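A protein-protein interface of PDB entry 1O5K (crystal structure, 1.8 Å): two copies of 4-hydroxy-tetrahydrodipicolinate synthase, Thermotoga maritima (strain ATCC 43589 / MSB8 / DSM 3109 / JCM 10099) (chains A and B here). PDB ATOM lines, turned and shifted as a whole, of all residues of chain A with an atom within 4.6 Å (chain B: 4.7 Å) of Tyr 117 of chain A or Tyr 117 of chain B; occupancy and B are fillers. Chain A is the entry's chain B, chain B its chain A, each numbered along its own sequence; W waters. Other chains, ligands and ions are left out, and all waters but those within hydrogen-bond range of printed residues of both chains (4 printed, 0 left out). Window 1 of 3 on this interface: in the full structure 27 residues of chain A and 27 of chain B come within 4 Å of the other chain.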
ATOM      1  N   GLY A  89      -4.468  21.485 -26.642  1.00  0.00           N
ATOM      2  CA  GLY A  89      -4.186  21.673 -25.240  1.00  0.00           C
ATOM      3  C   GLY A  89      -4.968  20.684 -24.414  1.00  0.00           C
ATOM      4  O   GLY A  89      -6.166  20.487 -24.657  1.00  0.00           O
ATOM      5  N   THR A  90      -4.317  20.046 -23.436  1.00  0.00           N
ATOM      6  CA  THR A  90      -5.056  19.252 -22.443  1.00  0.00           C
ATOM      7  C   THR A  90      -4.650  19.757 -21.064  1.00  0.00           C
ATOM      8  O   THR A  90      -3.887  20.736 -20.936  1.00  0.00           O
ATOM      9  CB  THR A  90      -4.818  17.729 -22.559  1.00  0.00           C
ATOM     10  OG1 THR A  90      -3.545  17.370 -21.995  1.00  0.00           O
ATOM     11  CG2 THR A  90      -4.753  17.243 -24.021  1.00  0.00           C
ATOM     12  N   ASN A  91      -5.099  19.061 -20.030  1.00  0.00           N
ATOM     13  CA  ASN A  91      -4.671  19.450 -18.655  1.00  0.00           C
ATOM     14  C   ASN A  91      -3.451  18.717 -18.126  1.00  0.00           C
ATOM     15  O   ASN A  91      -3.114  18.866 -16.947  1.00  0.00           O
ATOM     16  CB  ASN A  91      -5.837  19.369 -17.663  1.00  0.00           C
ATOM     17  CG  ASN A  91      -6.471  17.986 -17.583  1.00  0.00           C
ATOM     18  OD1 ASN A  91      -6.077  17.062 -18.336  1.00  0.00           O
ATOM     19  ND2 ASN A  91      -7.476  17.814 -16.658  1.00  0.00           N
ATOM     20  N   VAL A 114      -5.295  25.542 -24.854  1.00  0.00           N
ATOM     21  CA  VAL A 114      -6.082  26.028 -23.712  1.00  0.00           C
ATOM     22  C   VAL A 114      -5.298  25.865 -22.414  1.00  0.00           C
ATOM     23  O   VAL A 114      -4.463  24.961 -22.255  1.00  0.00           O
ATOM     24  CB  VAL A 114      -7.437  25.307 -23.628  1.00  0.00           C
ATOM     25  CG1 VAL A 114      -7.253  23.801 -23.223  1.00  0.00           C
ATOM     26  CG2 VAL A 114      -8.414  26.044 -22.699  1.00  0.00           C
ATOM     27  N   THR A 115      -5.488  26.814 -21.513  1.00  0.00           N
ATOM     28  CA  THR A 115      -5.008  26.607 -20.147  1.00  0.00           C
ATOM     29  C   THR A 115      -5.534  25.263 -19.599  1.00  0.00           C
ATOM     30  O   THR A 115      -6.714  24.989 -19.762  1.00  0.00           O
ATOM     31  CB  THR A 115      -5.492  27.669 -19.216  1.00  0.00           C
ATOM     32  OG1 THR A 115      -6.928  27.709 -19.172  1.00  0.00           O
ATOM     33  CG2 THR A 115      -5.072  29.013 -19.657  1.00  0.00           C
ATOM     34  N   PRO A 116      -4.698  24.454 -18.944  1.00  0.00           N
ATOM     35  CA  PRO A 116      -5.171  23.226 -18.274  1.00  0.00           C
ATOM     36  C   PRO A 116      -6.457  23.448 -17.495  1.00  0.00           C
ATOM     37  O   PRO A 116      -6.515  24.309 -16.627  1.00  0.00           O
ATOM     38  CB  PRO A 116      -4.035  22.868 -17.375  1.00  0.00           C
ATOM     39  CG  PRO A 116      -2.818  23.322 -18.172  1.00  0.00           C
ATOM     40  CD  PRO A 116      -3.215  24.564 -18.856  1.00  0.00           C
ATOM     41  N   TYR A 117      -7.486  22.680 -17.880  1.00  0.00           N
ATOM     42  CA  TYR A 117      -8.777  22.685 -17.238  1.00  0.00           C
ATOM     43  C   TYR A 117      -8.864  21.669 -16.102  1.00  0.00           C
ATOM     44  O   TYR A 117      -8.104  20.708 -16.062  1.00  0.00           O
ATOM     45  CB  TYR A 117      -9.872  22.338 -18.288  1.00  0.00           C
ATOM     46  CG  TYR A 117      -9.443  21.244 -19.241  1.00  0.00           C
ATOM     47  CD1 TYR A 117      -9.588  19.907 -18.901  1.00  0.00           C
ATOM     48  CD2 TYR A 117      -8.871  21.536 -20.464  1.00  0.00           C
ATOM     49  CE1 TYR A 117      -9.173  18.895 -19.755  1.00  0.00           C
ATOM     50  CE2 TYR A 117      -8.439  20.493 -21.354  1.00  0.00           C
ATOM     51  CZ  TYR A 117      -8.595  19.191 -20.970  1.00  0.00           C
ATOM     52  OH  TYR A 117      -8.199  18.158 -21.788  1.00  0.00           O
ATOM     53  N   TYR A 118      -9.803  21.908 -15.171  1.00  0.00           N
ATOM     54  CA  TYR A 118     -10.161  20.975 -14.106  1.00  0.00           C
ATOM     55  C   TYR A 118      -9.171  20.919 -12.954  1.00  0.00           C
ATOM     56  O   TYR A 118      -9.598  20.913 -11.825  1.00  0.00           O
ATOM     57  CB  TYR A 118     -10.422  19.602 -14.668  1.00  0.00           C
ATOM     58  CG  TYR A 118     -10.936  18.574 -13.683  1.00  0.00           C
ATOM     59  CD1 TYR A 118     -12.119  18.775 -12.983  1.00  0.00           C
ATOM     60  CD2 TYR A 118     -10.212  17.400 -13.442  1.00  0.00           C
ATOM     61  CE1 TYR A 118     -12.572  17.847 -12.108  1.00  0.00           C
ATOM     62  CE2 TYR A 118     -10.691  16.426 -12.565  1.00  0.00           C
ATOM     63  CZ  TYR A 118     -11.871  16.667 -11.892  1.00  0.00           C
ATOM     64  OH  TYR A 118     -12.373  15.738 -10.984  1.00  0.00           O
ATOM     65  N   ASN A 119      -7.872  20.898 -13.256  1.00  0.00           N
ATOM     66  CA  ASN A 119      -6.830  20.842 -12.208  1.00  0.00           C
ATOM     67  C   ASN A 119      -6.355  22.207 -11.687  1.00  0.00           C
ATOM     68  O   ASN A 119      -5.575  22.234 -10.773  1.00  0.00           O
ATOM     69  CB  ASN A 119      -5.630  19.912 -12.534  1.00  0.00           C
ATOM     70  CG  ASN A 119      -4.949  20.203 -13.860  1.00  0.00           C
ATOM     71  OD1 ASN A 119      -5.341  21.128 -14.599  1.00  0.00           O
ATOM     72  ND2 ASN A 119      -3.937  19.330 -14.217  1.00  0.00           N
ATOM     73  N   THR A 150     -12.789  26.261 -17.815  1.00  0.00           N
ATOM     74  CA  THR A 150     -11.607  25.569 -17.301  1.00  0.00           C
ATOM     75  C   THR A 150     -11.462  25.590 -15.796  1.00  0.00           C
ATOM     76  O   THR A 150     -10.752  24.766 -15.203  1.00  0.00           O
ATOM     77  CB  THR A 150     -10.333  26.239 -17.859  1.00  0.00           C
ATOM     78  OG1 THR A 150     -10.263  27.602 -17.391  1.00  0.00           O
ATOM     79  CG2 THR A 150     -10.327  26.212 -19.405  1.00  0.00           C
ATOM     80  N   GLY B  89     -13.625   9.264 -14.467  1.00  0.00           N
ATOM     81  CA  GLY B  89     -14.461  10.157 -15.279  1.00  0.00           C
ATOM     82  C   GLY B  89     -13.606  11.020 -16.193  1.00  0.00           C
ATOM     83  O   GLY B  89     -12.561  11.527 -15.779  1.00  0.00           O
ATOM     84  N   THR B  90     -14.034  11.187 -17.434  1.00  0.00           N
ATOM     85  CA  THR B  90     -13.450  12.200 -18.317  1.00  0.00           C
ATOM     86  C   THR B  90     -14.593  12.970 -18.983  1.00  0.00           C
ATOM     87  O   THR B  90     -15.758  12.784 -18.673  1.00  0.00           O
ATOM     88  CB  THR B  90     -12.483  11.611 -19.389  1.00  0.00           C
ATOM     89  OG1 THR B  90     -13.210  10.988 -20.497  1.00  0.00           O
ATOM     90  CG2 THR B  90     -11.626  10.498 -18.825  1.00  0.00           C
ATOM     91  N   ASN B  91     -14.251  13.823 -19.915  1.00  0.00           N
ATOM     92  CA  ASN B  91     -15.304  14.610 -20.599  1.00  0.00           C
ATOM     93  C   ASN B  91     -15.780  14.005 -21.903  1.00  0.00           C
ATOM     94  O   ASN B  91     -16.590  14.643 -22.631  1.00  0.00           O
ATOM     95  CB  ASN B  91     -14.866  16.072 -20.702  1.00  0.00           C
ATOM     96  CG  ASN B  91     -13.649  16.280 -21.544  1.00  0.00           C
ATOM     97  OD1 ASN B  91     -12.984  15.320 -21.976  1.00  0.00           O
ATOM     98  ND2 ASN B  91     -13.283  17.580 -21.748  1.00  0.00           N
ATOM     99  N   VAL B 114     -16.488  11.938 -12.371  1.00  0.00           N
ATOM    100  CA  VAL B 114     -16.760  13.351 -12.359  1.00  0.00           C
ATOM    101  C   VAL B 114     -17.661  13.703 -13.534  1.00  0.00           C
ATOM    102  O   VAL B 114     -17.598  13.084 -14.611  1.00  0.00           O
ATOM    103  CB  VAL B 114     -15.429  14.180 -12.373  1.00  0.00           C
ATOM    104  CG1 VAL B 114     -14.668  13.970 -13.646  1.00  0.00           C
ATOM    105  CG2 VAL B 114     -15.654  15.638 -11.999  1.00  0.00           C
ATOM    106  N   THR B 115     -18.533  14.668 -13.319  1.00  0.00           N
ATOM    107  CA  THR B 115     -19.241  15.280 -14.463  1.00  0.00           C
ATOM    108  C   THR B 115     -18.189  15.738 -15.472  1.00  0.00           C
ATOM    109  O   THR B 115     -17.161  16.320 -15.106  1.00  0.00           O
ATOM    110  CB  THR B 115     -20.026  16.542 -14.048  1.00  0.00           C
ATOM    111  OG1 THR B 115     -19.121  17.494 -13.499  1.00  0.00           O
ATOM    112  CG2 THR B 115     -21.075  16.259 -12.964  1.00  0.00           C
ATOM    113  N   PRO B 116     -18.420  15.473 -16.752  1.00  0.00           N
ATOM    114  CA  PRO B 116     -17.559  15.995 -17.792  1.00  0.00           C
ATOM    115  C   PRO B 116     -17.202  17.454 -17.584  1.00  0.00           C
ATOM    116  O   PRO B 116     -18.079  18.314 -17.394  1.00  0.00           O
ATOM    117  CB  PRO B 116     -18.383  15.813 -19.050  1.00  0.00           C
ATOM    118  CG  PRO B 116     -19.129  14.490 -18.738  1.00  0.00           C
ATOM    119  CD  PRO B 116     -19.497  14.608 -17.297  1.00  0.00           C
ATOM    120  N   TYR B 117     -15.891  17.704 -17.559  1.00  0.00           N
ATOM    121  CA  TYR B 117     -15.296  19.043 -17.362  1.00  0.00           C
ATOM    122  C   TYR B 117     -15.035  19.677 -18.737  1.00  0.00           C
ATOM    123  O   TYR B 117     -14.935  18.962 -19.719  1.00  0.00           O
ATOM    124  CB  TYR B 117     -13.956  18.954 -16.564  1.00  0.00           C
ATOM    125  CG  TYR B 117     -13.118  17.759 -16.971  1.00  0.00           C
ATOM    126  CD1 TYR B 117     -12.322  17.796 -18.137  1.00  0.00           C
ATOM    127  CD2 TYR B 117     -13.194  16.562 -16.276  1.00  0.00           C
ATOM    128  CE1 TYR B 117     -11.589  16.709 -18.539  1.00  0.00           C
ATOM    129  CE2 TYR B 117     -12.478  15.461 -16.698  1.00  0.00           C
ATOM    130  CZ  TYR B 117     -11.665  15.548 -17.823  1.00  0.00           C
ATOM    131  OH  TYR B 117     -10.979  14.438 -18.221  1.00  0.00           O
ATOM    132  N   TYR B 118     -15.052  21.002 -18.793  1.00  0.00           N
ATOM    133  CA  TYR B 118     -14.646  21.811 -19.939  1.00  0.00           C
ATOM    134  C   TYR B 118     -15.678  21.941 -21.068  1.00  0.00           C
ATOM    135  O   TYR B 118     -15.823  23.035 -21.618  1.00  0.00           O
ATOM    136  CB  TYR B 118     -13.324  21.297 -20.516  1.00  0.00           C
ATOM    137  CG  TYR B 118     -12.658  22.179 -21.568  1.00  0.00           C
ATOM    138  CD1 TYR B 118     -12.389  23.512 -21.337  1.00  0.00           C
ATOM    139  CD2 TYR B 118     -12.283  21.653 -22.790  1.00  0.00           C
ATOM    140  CE1 TYR B 118     -11.802  24.307 -22.310  1.00  0.00           C
ATOM    141  CE2 TYR B 118     -11.700  22.436 -23.757  1.00  0.00           C
ATOM    142  CZ  TYR B 118     -11.467  23.774 -23.512  1.00  0.00           C
ATOM    143  OH  TYR B 118     -10.871  24.552 -24.460  1.00  0.00           O
ATOM    144  N   ASN B 119     -16.397  20.867 -21.390  1.00  0.00           N
ATOM    145  CA  ASN B 119     -17.382  20.932 -22.478  1.00  0.00           C
ATOM    146  C   ASN B 119     -18.802  21.214 -22.004  1.00  0.00           C
ATOM    147  O   ASN B 119     -19.678  21.322 -22.855  1.00  0.00           O
ATOM    148  CB  ASN B 119     -17.302  19.726 -23.386  1.00  0.00           C
ATOM    149  CG  ASN B 119     -17.418  18.399 -22.668  1.00  0.00           C
ATOM    150  OD1 ASN B 119     -17.668  18.323 -21.467  1.00  0.00           O
ATOM    151  ND2 ASN B 119     -17.343  17.305 -23.476  1.00  0.00           N
ATOM    152  N   ARG B 149     -14.431  23.396 -10.580  1.00  0.00           N
ATOM    153  CA  ARG B 149     -13.419  22.788 -11.450  1.00  0.00           C
ATOM    154  C   ARG B 149     -13.919  22.443 -12.869  1.00  0.00           C
ATOM    155  O   ARG B 149     -13.130  22.502 -13.796  1.00  0.00           O
ATOM    156  CB  ARG B 149     -12.837  21.532 -10.855  1.00  0.00           C
ATOM    157  CG  ARG B 149     -12.033  21.731  -9.603  1.00  0.00           C
ATOM    158  CD  ARG B 149     -11.431  20.431  -9.092  1.00  0.00           C
ATOM    159  NE  ARG B 149     -10.606  20.566  -7.872  1.00  0.00           N
ATOM    160  CZ  ARG B 149      -9.276  20.628  -7.870  1.00  0.00           C
ATOM    161  NH1 ARG B 149      -8.571  20.715  -6.728  1.00  0.00           N
ATOM    162  NH2 ARG B 149      -8.653  20.618  -9.009  1.00  0.00           N
ATOM    163  N   THR B 150     -15.185  22.035 -13.004  1.00  0.00           N
ATOM    164  CA  THR B 150     -15.690  21.479 -14.257  1.00  0.00           C
ATOM    165  C   THR B 150     -16.387  22.460 -15.160  1.00  0.00           C
ATOM    166  O   THR B 150     -16.440  22.244 -16.397  1.00  0.00           O
ATOM    167  CB  THR B 150     -16.727  20.377 -13.953  1.00  0.00           C
ATOM    168  OG1 THR B 150     -17.815  20.982 -13.212  1.00  0.00           O
ATOM    169  CG2 THR B 150     -16.095  19.287 -13.105  1.00  0.00           C
HETATM  170  O   HOH W   1     -12.887  22.233 -16.565  1.00  0.00           O
HETATM  171  O   HOH W   2     -10.853  17.831 -23.261  1.00  0.00           O
HETATM  172  O   HOH W   3      -5.737  20.052  -9.031  1.00  0.00           O
HETATM  173  O   HOH W   4      -8.696  15.197 -16.511  1.00  0.00           O
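The guanidinium group (NH2) of Arg 149 of chain B is in hydrogen-bond range of the backbone carbonyl oxygen (O) of Tyr 118 of chain A (3.0 Å).
The side-chain amide nitrogen (ND2) of Asn 91 of chain A sits at hydrogen-bond distance from the backbone carbonyl oxygen (O) of Tyr 117 of chain A, at 3.0 Å.
The backbone NH of Tyr 118 of chain B lies within hydrogen-bond range of the backbone carbonyl oxygen of Thr 150 of chain B (3.0 Å).
The side-chain amide oxygen (OD1) of Asn 119 of chain B lies close to the backbone carbonyl oxygen (O) of Tyr 117 of chain B (3.3 Å).
O of Tyr 117 of chain A sits close to OD1 of Asn 119 of chain A.
The side-chain amide nitrogen (ND2) of Asn 119 of chain A sits at hydrogen-bond distance from the backbone carbonyl oxygen (O) of Asn 91 of chain A, 2.9 Å away.
The side-chain amide nitrogen of Asn 91 of chain B lies within hydrogen-bond range of the backbone carbonyl oxygen of Tyr 117 of chain B (3.0 Å).
Tyr 118 of chain B touches Val 114 of chain A (OH to CG2, 3.4 Å).
Tyr 117 of chain B touches Tyr 117 of chain A.
CG of Tyr 118 of chain B touches CD2 of Tyr 117 of chain A, 3.997 Å away.
OH of Tyr 118 of chain A touches CG2 of Val 114 of chain B (3.4 Å).
Tyr 117 of chain B touches Tyr 118 of chain A.
CG2 of Thr 150 of chain B touches CE1 of Tyr 118 of chain A (3.9 Å).
Arg 149 of chain B touches Asn 119 of chain A (NH2 to CA, 3.7 Å).
CE1 of Tyr 118 of chain B touches CG2 of Thr 150 of chain A (3.8 Å).
Thr 150 of chain A touches Arg 149 of chain B (O to O, 3.6 Å).
Of the printed residues of chain B, Tyr 117 of chain A touches Tyr 117 (3.5 Å) and Tyr 118 (3.997 Å).
Printed residues of chain A within 4 Å of Tyr 117 of chain B: Tyr 117 (3.5 Å) and Tyr 118 (3.98 Å).
Of the printed residues of chain B, Tyr 118 of chain A touches Val 114 (3.4 Å), Tyr 117 (3.98 Å), Arg 149 (3.0 Å) and Thr 150 (3.9 Å).
Of the printed residues of chain A, Tyr 118 of chain B touches Val 114, Tyr 117 and Thr 150.
Thr 115 of chain B touches none of the printed residues of chain A.
Of the 10 printed residues of chain A, 5 touch a printed residue of chain B.
Hydrophobic or aromatic side chains of chain A within 4 Å of the printed part of chain B: Val 114, Tyr 117 and Tyr 118.
Of the 11 printed residues of chain B, 5 touch a printed residue of chain A.
Printed residues of chain B that touch a printed residue of chain A: Val 114, Tyr 117, Tyr 118, Arg 149 and Thr 150.
Hydrophobic or aromatic side chains of chain B within 4 Å of the printed part of chain A: Val 114, Tyr 117 and Tyr 118.
Among the printed residues, 10 pairs touch across the chains.
Among the printed residues, no Asp or Glu carboxylate lies within 4 Å of a Lys or Arg side-chain nitrogen of the other chain.
Val 114 of chain A touches Tyr 118 of chain B, and with the chains exchanged Tyr 118 of chain A touches Val 114 of chain B.
Tyr 117 of chain A touches its own counterpart, Tyr 117 of chain B.
Tyr 117 of chain A touches Tyr 118 of chain B, and with the chains exchanged Tyr 118 of chain A touches Tyr 117 of chain B.
Tyr 118 of chain A touches Thr 150 of chain B, and with the chains exchanged Thr 150 of chain A touches Tyr 118 of chain B.
Positions printed for both chains: 89, 90, 91, 114, 115, 116, 117, 118, 119 and 150.
Of the 10 pairs that touch across the chains among the printed residues, 7 have their exchanged pair printed and touching as well.
Water W1 lies within hydrogen-bond range of the backbone carbonyl oxygen (O) of Arg 149 of chain B (2.8 Å), the backbone NH (N) of Tyr 118 of chain B (3.3 Å) and the backbone NH (N) of Tyr 118 of chain A (3.4 Å).
Water W3 bridges the backbone carbonyl oxygen (O) of Asn 119 of chain A (2.8 Å) and the guanidinium group (NH2) of Arg 149 of chain B (3.0 Å).
Water W2 bridges the side-chain amide nitrogen (ND2) of Asn 91 of chain B (2.9 Å) and the side-chain hydroxyl (OH) of Tyr 117 of chain A (3.1 Å).
Water W4 lies within hydrogen-bond range of the side-chain amide nitrogen (ND2) of Asn 91 of chain A (2.9 Å) and the side-chain hydroxyl (OH) of Tyr 117 of chain B (3.0 Å).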
